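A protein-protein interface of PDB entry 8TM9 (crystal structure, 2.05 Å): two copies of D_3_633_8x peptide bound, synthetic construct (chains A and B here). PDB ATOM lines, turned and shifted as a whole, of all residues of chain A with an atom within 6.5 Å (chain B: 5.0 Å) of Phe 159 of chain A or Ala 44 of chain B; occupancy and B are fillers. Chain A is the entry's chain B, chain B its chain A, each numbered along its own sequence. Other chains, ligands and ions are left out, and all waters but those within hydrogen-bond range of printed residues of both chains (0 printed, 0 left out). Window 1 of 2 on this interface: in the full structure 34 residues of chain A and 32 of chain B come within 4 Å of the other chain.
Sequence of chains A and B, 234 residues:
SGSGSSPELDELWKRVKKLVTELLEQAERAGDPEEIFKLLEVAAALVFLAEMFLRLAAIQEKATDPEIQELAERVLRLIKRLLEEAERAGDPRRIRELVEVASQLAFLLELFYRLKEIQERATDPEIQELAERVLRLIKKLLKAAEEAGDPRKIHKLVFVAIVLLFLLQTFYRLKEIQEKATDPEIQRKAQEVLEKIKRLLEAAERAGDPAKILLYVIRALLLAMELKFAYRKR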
ATOM      1  N   GLN A 104      19.581 -35.650  26.047  1.00  0.00           N
ATOM      2  CA  GLN A 104      21.017 -35.531  26.281  1.00  0.00           C
ATOM      3  C   GLN A 104      21.647 -36.900  26.504  1.00  0.00           C
ATOM      4  O   GLN A 104      22.765 -37.161  26.046  1.00  0.00           O
ATOM      5  CB  GLN A 104      21.287 -34.616  27.478  1.00  0.00           C
ATOM      6  CG  GLN A 104      20.763 -33.199  27.311  1.00  0.00           C
ATOM      7  CD  GLN A 104      20.638 -32.457  28.628  1.00  0.00           C
ATOM      8  OE1 GLN A 104      21.227 -32.851  29.634  1.00  0.00           O
ATOM      9  NE2 GLN A 104      19.870 -31.374  28.626  1.00  0.00           N
ATOM     10  N   ILE A 154      21.232 -35.199  37.230  1.00  0.00           N
ATOM     11  CA  ILE A 154      21.549 -36.110  36.134  1.00  0.00           C
ATOM     12  C   ILE A 154      22.053 -35.332  34.926  1.00  0.00           C
ATOM     13  O   ILE A 154      23.000 -35.751  34.250  1.00  0.00           O
ATOM     14  CB  ILE A 154      20.321 -36.971  35.781  1.00  0.00           C
ATOM     15  CG1 ILE A 154      19.894 -37.814  36.982  1.00  0.00           C
ATOM     16  CG2 ILE A 154      20.618 -37.866  34.587  1.00  0.00           C
ATOM     17  CD1 ILE A 154      18.670 -38.664  36.721  1.00  0.00           C
ATOM     18  N   HIS A 155      21.434 -34.183  34.642  1.00  0.00           N
ATOM     19  CA  HIS A 155      21.858 -33.369  33.507  1.00  0.00           C
ATOM     20  C   HIS A 155      23.311 -32.933  33.648  1.00  0.00           C
ATOM     21  O   HIS A 155      24.058 -32.913  32.663  1.00  0.00           O
ATOM     22  CB  HIS A 155      20.949 -32.150  33.364  1.00  0.00           C
ATOM     23  CG  HIS A 155      21.604 -30.989  32.684  1.00  0.00           C
ATOM     24  ND1 HIS A 155      21.824 -30.950  31.324  1.00  0.00           N
ATOM     25  CD2 HIS A 155      22.097 -29.828  33.178  1.00  0.00           C
ATOM     26  CE1 HIS A 155      22.420 -29.814  31.009  1.00  0.00           C
ATOM     27  NE2 HIS A 155      22.597 -29.115  32.115  1.00  0.00           N
ATOM     28  N   LYS A 156      23.730 -32.580  34.866  1.00  0.00           N
ATOM     29  CA  LYS A 156      25.110 -32.159  35.082  1.00  0.00           C
ATOM     30  C   LYS A 156      26.079 -33.304  34.817  1.00  0.00           C
ATOM     31  O   LYS A 156      27.109 -33.123  34.158  1.00  0.00           O
ATOM     32  CB  LYS A 156      25.282 -31.632  36.507  1.00  0.00           C
ATOM     33  CG  LYS A 156      24.676 -30.260  36.745  1.00  0.00           C
ATOM     34  CD  LYS A 156      24.792 -29.861  38.208  1.00  0.00           C
ATOM     35  CE  LYS A 156      24.356 -28.423  38.425  1.00  0.00           C
ATOM     36  NZ  LYS A 156      22.874 -28.305  38.522  1.00  0.00           N
ATOM     37  N   LEU A 157      25.761 -34.498  35.324  1.00  0.00           N
ATOM     38  CA  LEU A 157      26.651 -35.640  35.145  1.00  0.00           C
ATOM     39  C   LEU A 157      26.703 -36.080  33.687  1.00  0.00           C
ATOM     40  O   LEU A 157      27.761 -36.487  33.194  1.00  0.00           O
ATOM     41  CB  LEU A 157      26.202 -36.794  36.041  1.00  0.00           C
ATOM     42  CG  LEU A 157      26.180 -36.501  37.543  1.00  0.00           C
ATOM     43  CD1 LEU A 157      25.178 -37.396  38.255  1.00  0.00           C
ATOM     44  CD2 LEU A 157      27.569 -36.665  38.141  1.00  0.00           C
ATOM     45  N   VAL A 158      25.572 -36.004  32.983  1.00  0.00           N
ATOM     46  CA  VAL A 158      25.551 -36.377  31.572  1.00  0.00           C
ATOM     47  C   VAL A 158      26.279 -35.334  30.734  1.00  0.00           C
ATOM     48  O   VAL A 158      26.976 -35.669  29.768  1.00  0.00           O
ATOM     49  CB  VAL A 158      24.099 -36.581  31.101  1.00  0.00           C
ATOM     50  CG1 VAL A 158      24.038 -36.752  29.591  1.00  0.00           C
ATOM     51  CG2 VAL A 158      23.485 -37.784  31.801  1.00  0.00           C
ATOM     52  N   PHE A 159      26.135 -34.054  31.092  1.00  0.00           N
ATOM     53  CA  PHE A 159      26.850 -32.998  30.380  1.00  0.00           C
ATOM     54  C   PHE A 159      28.357 -33.204  30.457  1.00  0.00           C
ATOM     55  O   PHE A 159      29.066 -33.038  29.459  1.00  0.00           O
ATOM     56  CB  PHE A 159      26.468 -31.632  30.950  1.00  0.00           C
ATOM     57  CG  PHE A 159      26.964 -30.471  30.134  1.00  0.00           C
ATOM     58  CD1 PHE A 159      28.211 -29.917  30.374  1.00  0.00           C
ATOM     59  CD2 PHE A 159      26.180 -29.930  29.131  1.00  0.00           C
ATOM     60  CE1 PHE A 159      28.667 -28.849  29.622  1.00  0.00           C
ATOM     61  CE2 PHE A 159      26.628 -28.865  28.377  1.00  0.00           C
ATOM     62  CZ  PHE A 159      27.873 -28.323  28.623  1.00  0.00           C
ATOM     63  N   VAL A 160      28.864 -33.569  31.637  1.00  0.00           N
ATOM     64  CA  VAL A 160      30.296 -33.808  31.791  1.00  0.00           C
ATOM     65  C   VAL A 160      30.725 -35.016  30.968  1.00  0.00           C
ATOM     66  O   VAL A 160      31.806 -35.024  30.365  1.00  0.00           O
ATOM     67  CB  VAL A 160      30.649 -33.977  33.281  1.00  0.00           C
ATOM     68  CG1 VAL A 160      32.118 -34.323  33.446  1.00  0.00           C
ATOM     69  CG2 VAL A 160      30.308 -32.711  34.053  1.00  0.00           C
ATOM     70  N   ALA A 161      29.885 -36.052  30.920  1.00  0.00           N
ATOM     71  CA  ALA A 161      30.212 -37.228  30.121  1.00  0.00           C
ATOM     72  C   ALA A 161      30.241 -36.895  28.634  1.00  0.00           C
ATOM     73  O   ALA A 161      31.054 -37.447  27.884  1.00  0.00           O
ATOM     74  CB  ALA A 161      29.212 -38.350  30.402  1.00  0.00           C
ATOM     75  N   ILE A 162      29.366 -35.989  28.193  1.00  0.00           N
ATOM     76  CA  ILE A 162      29.327 -35.614  26.782  1.00  0.00           C
ATOM     77  C   ILE A 162      30.590 -34.853  26.394  1.00  0.00           C
ATOM     78  O   ILE A 162      31.210 -35.133  25.362  1.00  0.00           O
ATOM     79  CB  ILE A 162      28.058 -34.794  26.482  1.00  0.00           C
ATOM     80  CG1 ILE A 162      26.816 -35.686  26.550  1.00  0.00           C
ATOM     81  CG2 ILE A 162      28.160 -34.124  25.120  1.00  0.00           C
ATOM     82  CD1 ILE A 162      25.513 -34.919  26.518  1.00  0.00           C
ATOM     83  N   VAL A 163      30.994 -33.882  27.217  1.00  0.00           N
ATOM     84  CA  VAL A 163      32.175 -33.092  26.880  1.00  0.00           C
ATOM     85  C   VAL A 163      33.444 -33.919  27.037  1.00  0.00           C
ATOM     86  O   VAL A 163      34.459 -33.637  26.388  1.00  0.00           O
ATOM     87  CB  VAL A 163      32.226 -31.805  27.726  1.00  0.00           C
ATOM     88  CG1 VAL A 163      30.953 -30.994  27.534  1.00  0.00           C
ATOM     89  CG2 VAL A 163      32.447 -32.129  29.193  1.00  0.00           C
ATOM     90  N   LEU A 164      33.419 -34.948  27.889  1.00  0.00           N
ATOM     91  CA  LEU A 164      34.558 -35.854  27.979  1.00  0.00           C
ATOM     92  C   LEU A 164      34.724 -36.650  26.691  1.00  0.00           C
ATOM     93  O   LEU A 164      35.851 -36.900  26.249  1.00  0.00           O
ATOM     94  CB  LEU A 164      34.393 -36.797  29.170  1.00  0.00           C
ATOM     95  CG  LEU A 164      34.944 -36.323  30.515  1.00  0.00           C
ATOM     96  CD1 LEU A 164      34.416 -37.198  31.641  1.00  0.00           C
ATOM     97  CD2 LEU A 164      36.466 -36.322  30.501  1.00  0.00           C
ATOM     98  N   PHE A 166      33.745 -35.509  23.780  1.00  0.00           N
ATOM     99  CA  PHE A 166      34.305 -34.502  22.885  1.00  0.00           C
ATOM    100  C   PHE A 166      35.818 -34.422  23.047  1.00  0.00           C
ATOM    101  O   PHE A 166      36.557 -34.388  22.056  1.00  0.00           O
ATOM    102  CB  PHE A 166      33.650 -33.144  23.160  1.00  0.00           C
ATOM    103  CG  PHE A 166      33.998 -32.064  22.159  1.00  0.00           C
ATOM    104  CD1 PHE A 166      34.660 -32.360  20.976  1.00  0.00           C
ATOM    105  CD2 PHE A 166      33.666 -30.743  22.416  1.00  0.00           C
ATOM    106  CE1 PHE A 166      34.979 -31.363  20.071  1.00  0.00           C
ATOM    107  CE2 PHE A 166      33.980 -29.743  21.514  1.00  0.00           C
ATOM    108  CZ  PHE A 166      34.638 -30.055  20.341  1.00  0.00           C
ATOM    109  N   LEU A 214      34.470 -30.597  34.535  1.00  0.00           N
ATOM    110  CA  LEU A 214      34.033 -29.840  33.366  1.00  0.00           C
ATOM    111  C   LEU A 214      34.982 -28.685  33.069  1.00  0.00           C
ATOM    112  O   LEU A 214      35.289 -28.408  31.904  1.00  0.00           O
ATOM    113  CB  LEU A 214      32.609 -29.328  33.583  1.00  0.00           C
ATOM    114  CG  LEU A 214      32.009 -28.408  32.517  1.00  0.00           C
ATOM    115  CD1 LEU A 214      32.072 -29.056  31.144  1.00  0.00           C
ATOM    116  CD2 LEU A 214      30.578 -28.049  32.878  1.00  0.00           C
ATOM    117  N   ILE A 218      37.059 -28.243  29.540  1.00  0.00           N
ATOM    118  CA  ILE A 218      36.912 -27.055  28.701  1.00  0.00           C
ATOM    119  C   ILE A 218      38.273 -26.432  28.418  1.00  0.00           C
ATOM    120  O   ILE A 218      38.550 -25.990  27.296  1.00  0.00           O
ATOM    121  CB  ILE A 218      35.951 -26.047  29.359  1.00  0.00           C
ATOM    122  CG1 ILE A 218      34.531 -26.612  29.405  1.00  0.00           C
ATOM    123  CG2 ILE A 218      35.963 -24.721  28.610  1.00  0.00           C
ATOM    124  CD1 ILE A 218      33.594 -25.807  30.273  1.00  0.00           C
ATOM    125  N   LEU A 221      39.846 -28.635  25.771  1.00  0.00           N
ATOM    126  CA  LEU A 221      39.235 -28.426  24.463  1.00  0.00           C
ATOM    127  C   LEU A 221      39.594 -27.063  23.889  1.00  0.00           C
ATOM    128  O   LEU A 221      39.706 -26.917  22.665  1.00  0.00           O
ATOM    129  CB  LEU A 221      37.717 -28.578  24.565  1.00  0.00           C
ATOM    130  CG  LEU A 221      37.200 -29.995  24.820  1.00  0.00           C
ATOM    131  CD1 LEU A 221      35.760 -29.967  25.310  1.00  0.00           C
ATOM    132  CD2 LEU A 221      37.326 -30.840  23.564  1.00  0.00           C
ATOM    133  N   PHE B  37      28.332 -24.028  37.240  1.00  0.00           N
ATOM    134  CA  PHE B  37      28.106 -25.029  36.203  1.00  0.00           C
ATOM    135  C   PHE B  37      27.403 -24.427  34.993  1.00  0.00           C
ATOM    136  O   PHE B  37      27.747 -24.745  33.849  1.00  0.00           O
ATOM    137  CB  PHE B  37      27.300 -26.200  36.765  1.00  0.00           C
ATOM    138  CG  PHE B  37      27.451 -27.468  35.973  1.00  0.00           C
ATOM    139  CD1 PHE B  37      26.649 -27.712  34.870  1.00  0.00           C
ATOM    140  CD2 PHE B  37      28.402 -28.410  36.326  1.00  0.00           C
ATOM    141  CE1 PHE B  37      26.790 -28.876  34.137  1.00  0.00           C
ATOM    142  CE2 PHE B  37      28.549 -29.576  35.596  1.00  0.00           C
ATOM    143  CZ  PHE B  37      27.742 -29.808  34.501  1.00  0.00           C
ATOM    144  N   LEU B  40      29.900 -22.562  32.927  1.00  0.00           N
ATOM    145  CA  LEU B  40      30.774 -23.480  32.207  1.00  0.00           C
ATOM    146  C   LEU B  40      30.044 -24.165  31.059  1.00  0.00           C
ATOM    147  O   LEU B  40      30.668 -24.512  30.050  1.00  0.00           O
ATOM    148  CB  LEU B  40      31.351 -24.519  33.168  1.00  0.00           C
ATOM    149  CG  LEU B  40      32.350 -24.009  34.208  1.00  0.00           C
ATOM    150  CD1 LEU B  40      32.621 -25.073  35.261  1.00  0.00           C
ATOM    151  CD2 LEU B  40      33.643 -23.570  33.539  1.00  0.00           C
ATOM    152  N   GLU B  41      28.729 -24.368  31.190  1.00  0.00           N
ATOM    153  CA  GLU B  41      27.962 -24.970  30.104  1.00  0.00           C
ATOM    154  C   GLU B  41      27.969 -24.083  28.867  1.00  0.00           C
ATOM    155  O   GLU B  41      28.072 -24.579  27.739  1.00  0.00           O
ATOM    156  CB  GLU B  41      26.526 -25.237  30.556  1.00  0.00           C
ATOM    157  CG  GLU B  41      26.366 -26.434  31.477  1.00  0.00           C
ATOM    158  CD  GLU B  41      24.931 -26.628  31.928  1.00  0.00           C
ATOM    159  OE1 GLU B  41      24.556 -27.775  32.249  1.00  0.00           O
ATOM    160  OE2 GLU B  41      24.176 -25.633  31.960  1.00  0.00           O
ATOM    161  N   VAL B  42      27.852 -22.768  29.056  1.00  0.00           N
ATOM    162  CA  VAL B  42      27.878 -21.855  27.918  1.00  0.00           C
ATOM    163  C   VAL B  42      29.275 -21.802  27.313  1.00  0.00           C
ATOM    164  O   VAL B  42      29.432 -21.702  26.091  1.00  0.00           O
ATOM    165  CB  VAL B  42      27.385 -20.457  28.336  1.00  0.00           C
ATOM    166  CG1 VAL B  42      27.121 -19.600  27.106  1.00  0.00           C
ATOM    167  CG2 VAL B  42      26.132 -20.568  29.189  1.00  0.00           C
ATOM    168  N   ALA B  43      30.309 -21.866  28.155  1.00  0.00           N
ATOM    169  CA  ALA B  43      31.675 -21.921  27.645  1.00  0.00           C
ATOM    170  C   ALA B  43      31.899 -23.180  26.818  1.00  0.00           C
ATOM    171  O   ALA B  43      32.541 -23.134  25.763  1.00  0.00           O
ATOM    172  CB  ALA B  43      32.673 -21.851  28.801  1.00  0.00           C
ATOM    173  N   ALA B  44      31.373 -24.317  27.283  1.00  0.00           N
ATOM    174  CA  ALA B  44      31.465 -25.543  26.498  1.00  0.00           C
ATOM    175  C   ALA B  44      30.676 -25.423  25.202  1.00  0.00           C
ATOM    176  O   ALA B  44      31.105 -25.924  24.156  1.00  0.00           O
ATOM    177  CB  ALA B  44      30.973 -26.734  27.320  1.00  0.00           C
ATOM    178  N   ALA B  45      29.519 -24.756  25.251  1.00  0.00           N
ATOM    179  CA  ALA B  45      28.712 -24.577  24.047  1.00  0.00           C
ATOM    180  C   ALA B  45      29.449 -23.742  23.008  1.00  0.00           C
ATOM    181  O   ALA B  45      29.335 -23.994  21.803  1.00  0.00           O
ATOM    182  CB  ALA B  45      27.373 -23.931  24.401  1.00  0.00           C
ATOM    183  N   LEU B  46      30.208 -22.741  23.455  1.00  0.00           N
ATOM    184  CA  LEU B  46      30.962 -21.916  22.518  1.00  0.00           C
ATOM    185  C   LEU B  46      32.105 -22.700  21.886  1.00  0.00           C
ATOM    186  O   LEU B  46      32.416 -22.509  20.705  1.00  0.00           O
ATOM    187  CB  LEU B  46      31.490 -20.673  23.227  1.00  0.00           C
ATOM    188  CG  LEU B  46      30.524 -19.495  23.327  1.00  0.00           C
ATOM    189  CD1 LEU B  46      30.852 -18.669  24.548  1.00  0.00           C
ATOM    190  CD2 LEU B  46      30.591 -18.643  22.073  1.00  0.00           C
ATOM    191  N   VAL B  47      32.742 -23.584  22.656  1.00  0.00           N
ATOM    192  CA  VAL B  47      33.797 -24.422  22.095  1.00  0.00           C
ATOM    193  C   VAL B  47      33.222 -25.370  21.051  1.00  0.00           C
ATOM    194  O   VAL B  47      33.835 -25.606  20.003  1.00  0.00           O
ATOM    195  CB  VAL B  47      34.532 -25.182  23.214  1.00  0.00           C
ATOM    196  CG1 VAL B  47      35.603 -26.088  22.625  1.00  0.00           C
ATOM    197  CG2 VAL B  47      35.151 -24.203  24.196  1.00  0.00           C
ATOM    198  N   PHE B  48      32.034 -25.922  21.310  1.00  0.00           N
ATOM    199  CA  PHE B  48      31.404 -26.787  20.320  1.00  0.00           C
ATOM    200  C   PHE B  48      30.990 -26.006  19.080  1.00  0.00           C
ATOM    201  O   PHE B  48      31.003 -26.557  17.972  1.00  0.00           O
ATOM    202  CB  PHE B  48      30.197 -27.503  20.927  1.00  0.00           C
ATOM    203  CG  PHE B  48      29.449 -28.366  19.949  1.00  0.00           C
ATOM    204  CD1 PHE B  48      29.788 -29.698  19.786  1.00  0.00           C
ATOM    205  CD2 PHE B  48      28.403 -27.850  19.201  1.00  0.00           C
ATOM    206  CE1 PHE B  48      29.107 -30.497  18.887  1.00  0.00           C
ATOM    207  CE2 PHE B  48      27.722 -28.643  18.300  1.00  0.00           C
ATOM    208  CZ  PHE B  48      28.070 -29.967  18.145  1.00  0.00           C
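Phe 159 of chain A touches just these residues of chain B: Glu 41 and Ala 44. Printed residues of chain A within 4 Å of Ala 44 of chain B: Phe 159 (3.7 Å). Of the printed residues of chain A, Val 47 of chain B touches Leu 221. Printed residues of chain B within 4 Å of His 155 of chain A: Glu 41. Of the printed residues of chain A, Leu 40 of chain B touches Leu 214 and Ile 218. The nearest printed residue of chain B that does not touch Ile 218 of chain A is Ala 44 of chain B (4.01 Å).
A ring nitrogen (NE2) of His 155 of chain A lies close to the side-chain carboxylate (OE1) of Glu 41 of chain B (2.4 Å).
ND1 of His 155 of chain A sits at hydrogen-bond distance from OE1 of Gln 104 of chain A (2.6 Å).
Hydrophobic or aromatic side chains of chain B within 4 Å of the printed part of chain A: Phe 37, Leu 40, Ala 44 and Val 47. Of the 16 printed residues of chain A, 7 touch a printed residue of chain B. Printed residues of chain A that touch a printed residue of chain B: His 155, Lys 156, Phe 159, Val 160, Leu 214, Ile 218 and Leu 221. Hydrophobic or aromatic side chains of chain A within 4 Å of the printed part of chain B: His 155, Phe 159, Val 160, Leu 214, Ile 218 and Leu 221. Among the printed residues, no Asp or Glu carboxylate lies within 4 Å of a Lys or Arg side-chain nitrogen of the other chain.
No position is printed for both chains. Of the 9 pairs that touch across the chains among the printed residues, none has its exchanged pair printed and touching as well.
Among the printed residues, merely in contact across the chains: Ile 218 of chain A with Leu 40 of chain B (3.2 Å), Lys 156 of chain A with Phe 37 of chain B (3.4 Å), Leu 214 of chain A with Leu 40 of chain B (3.6 Å), Phe 159 of chain A with Glu 41 of chain B (3.7 Å), Leu 214 of chain A with Phe 37 of chain B (3.7 Å), Phe 159 of chain A with Ala 44 of chain B (3.7 Å), Leu 221 of chain A with Val 47 of chain B (3.8 Å) and Val 160 of chain A with Phe 37 of chain B (3.9 Å).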
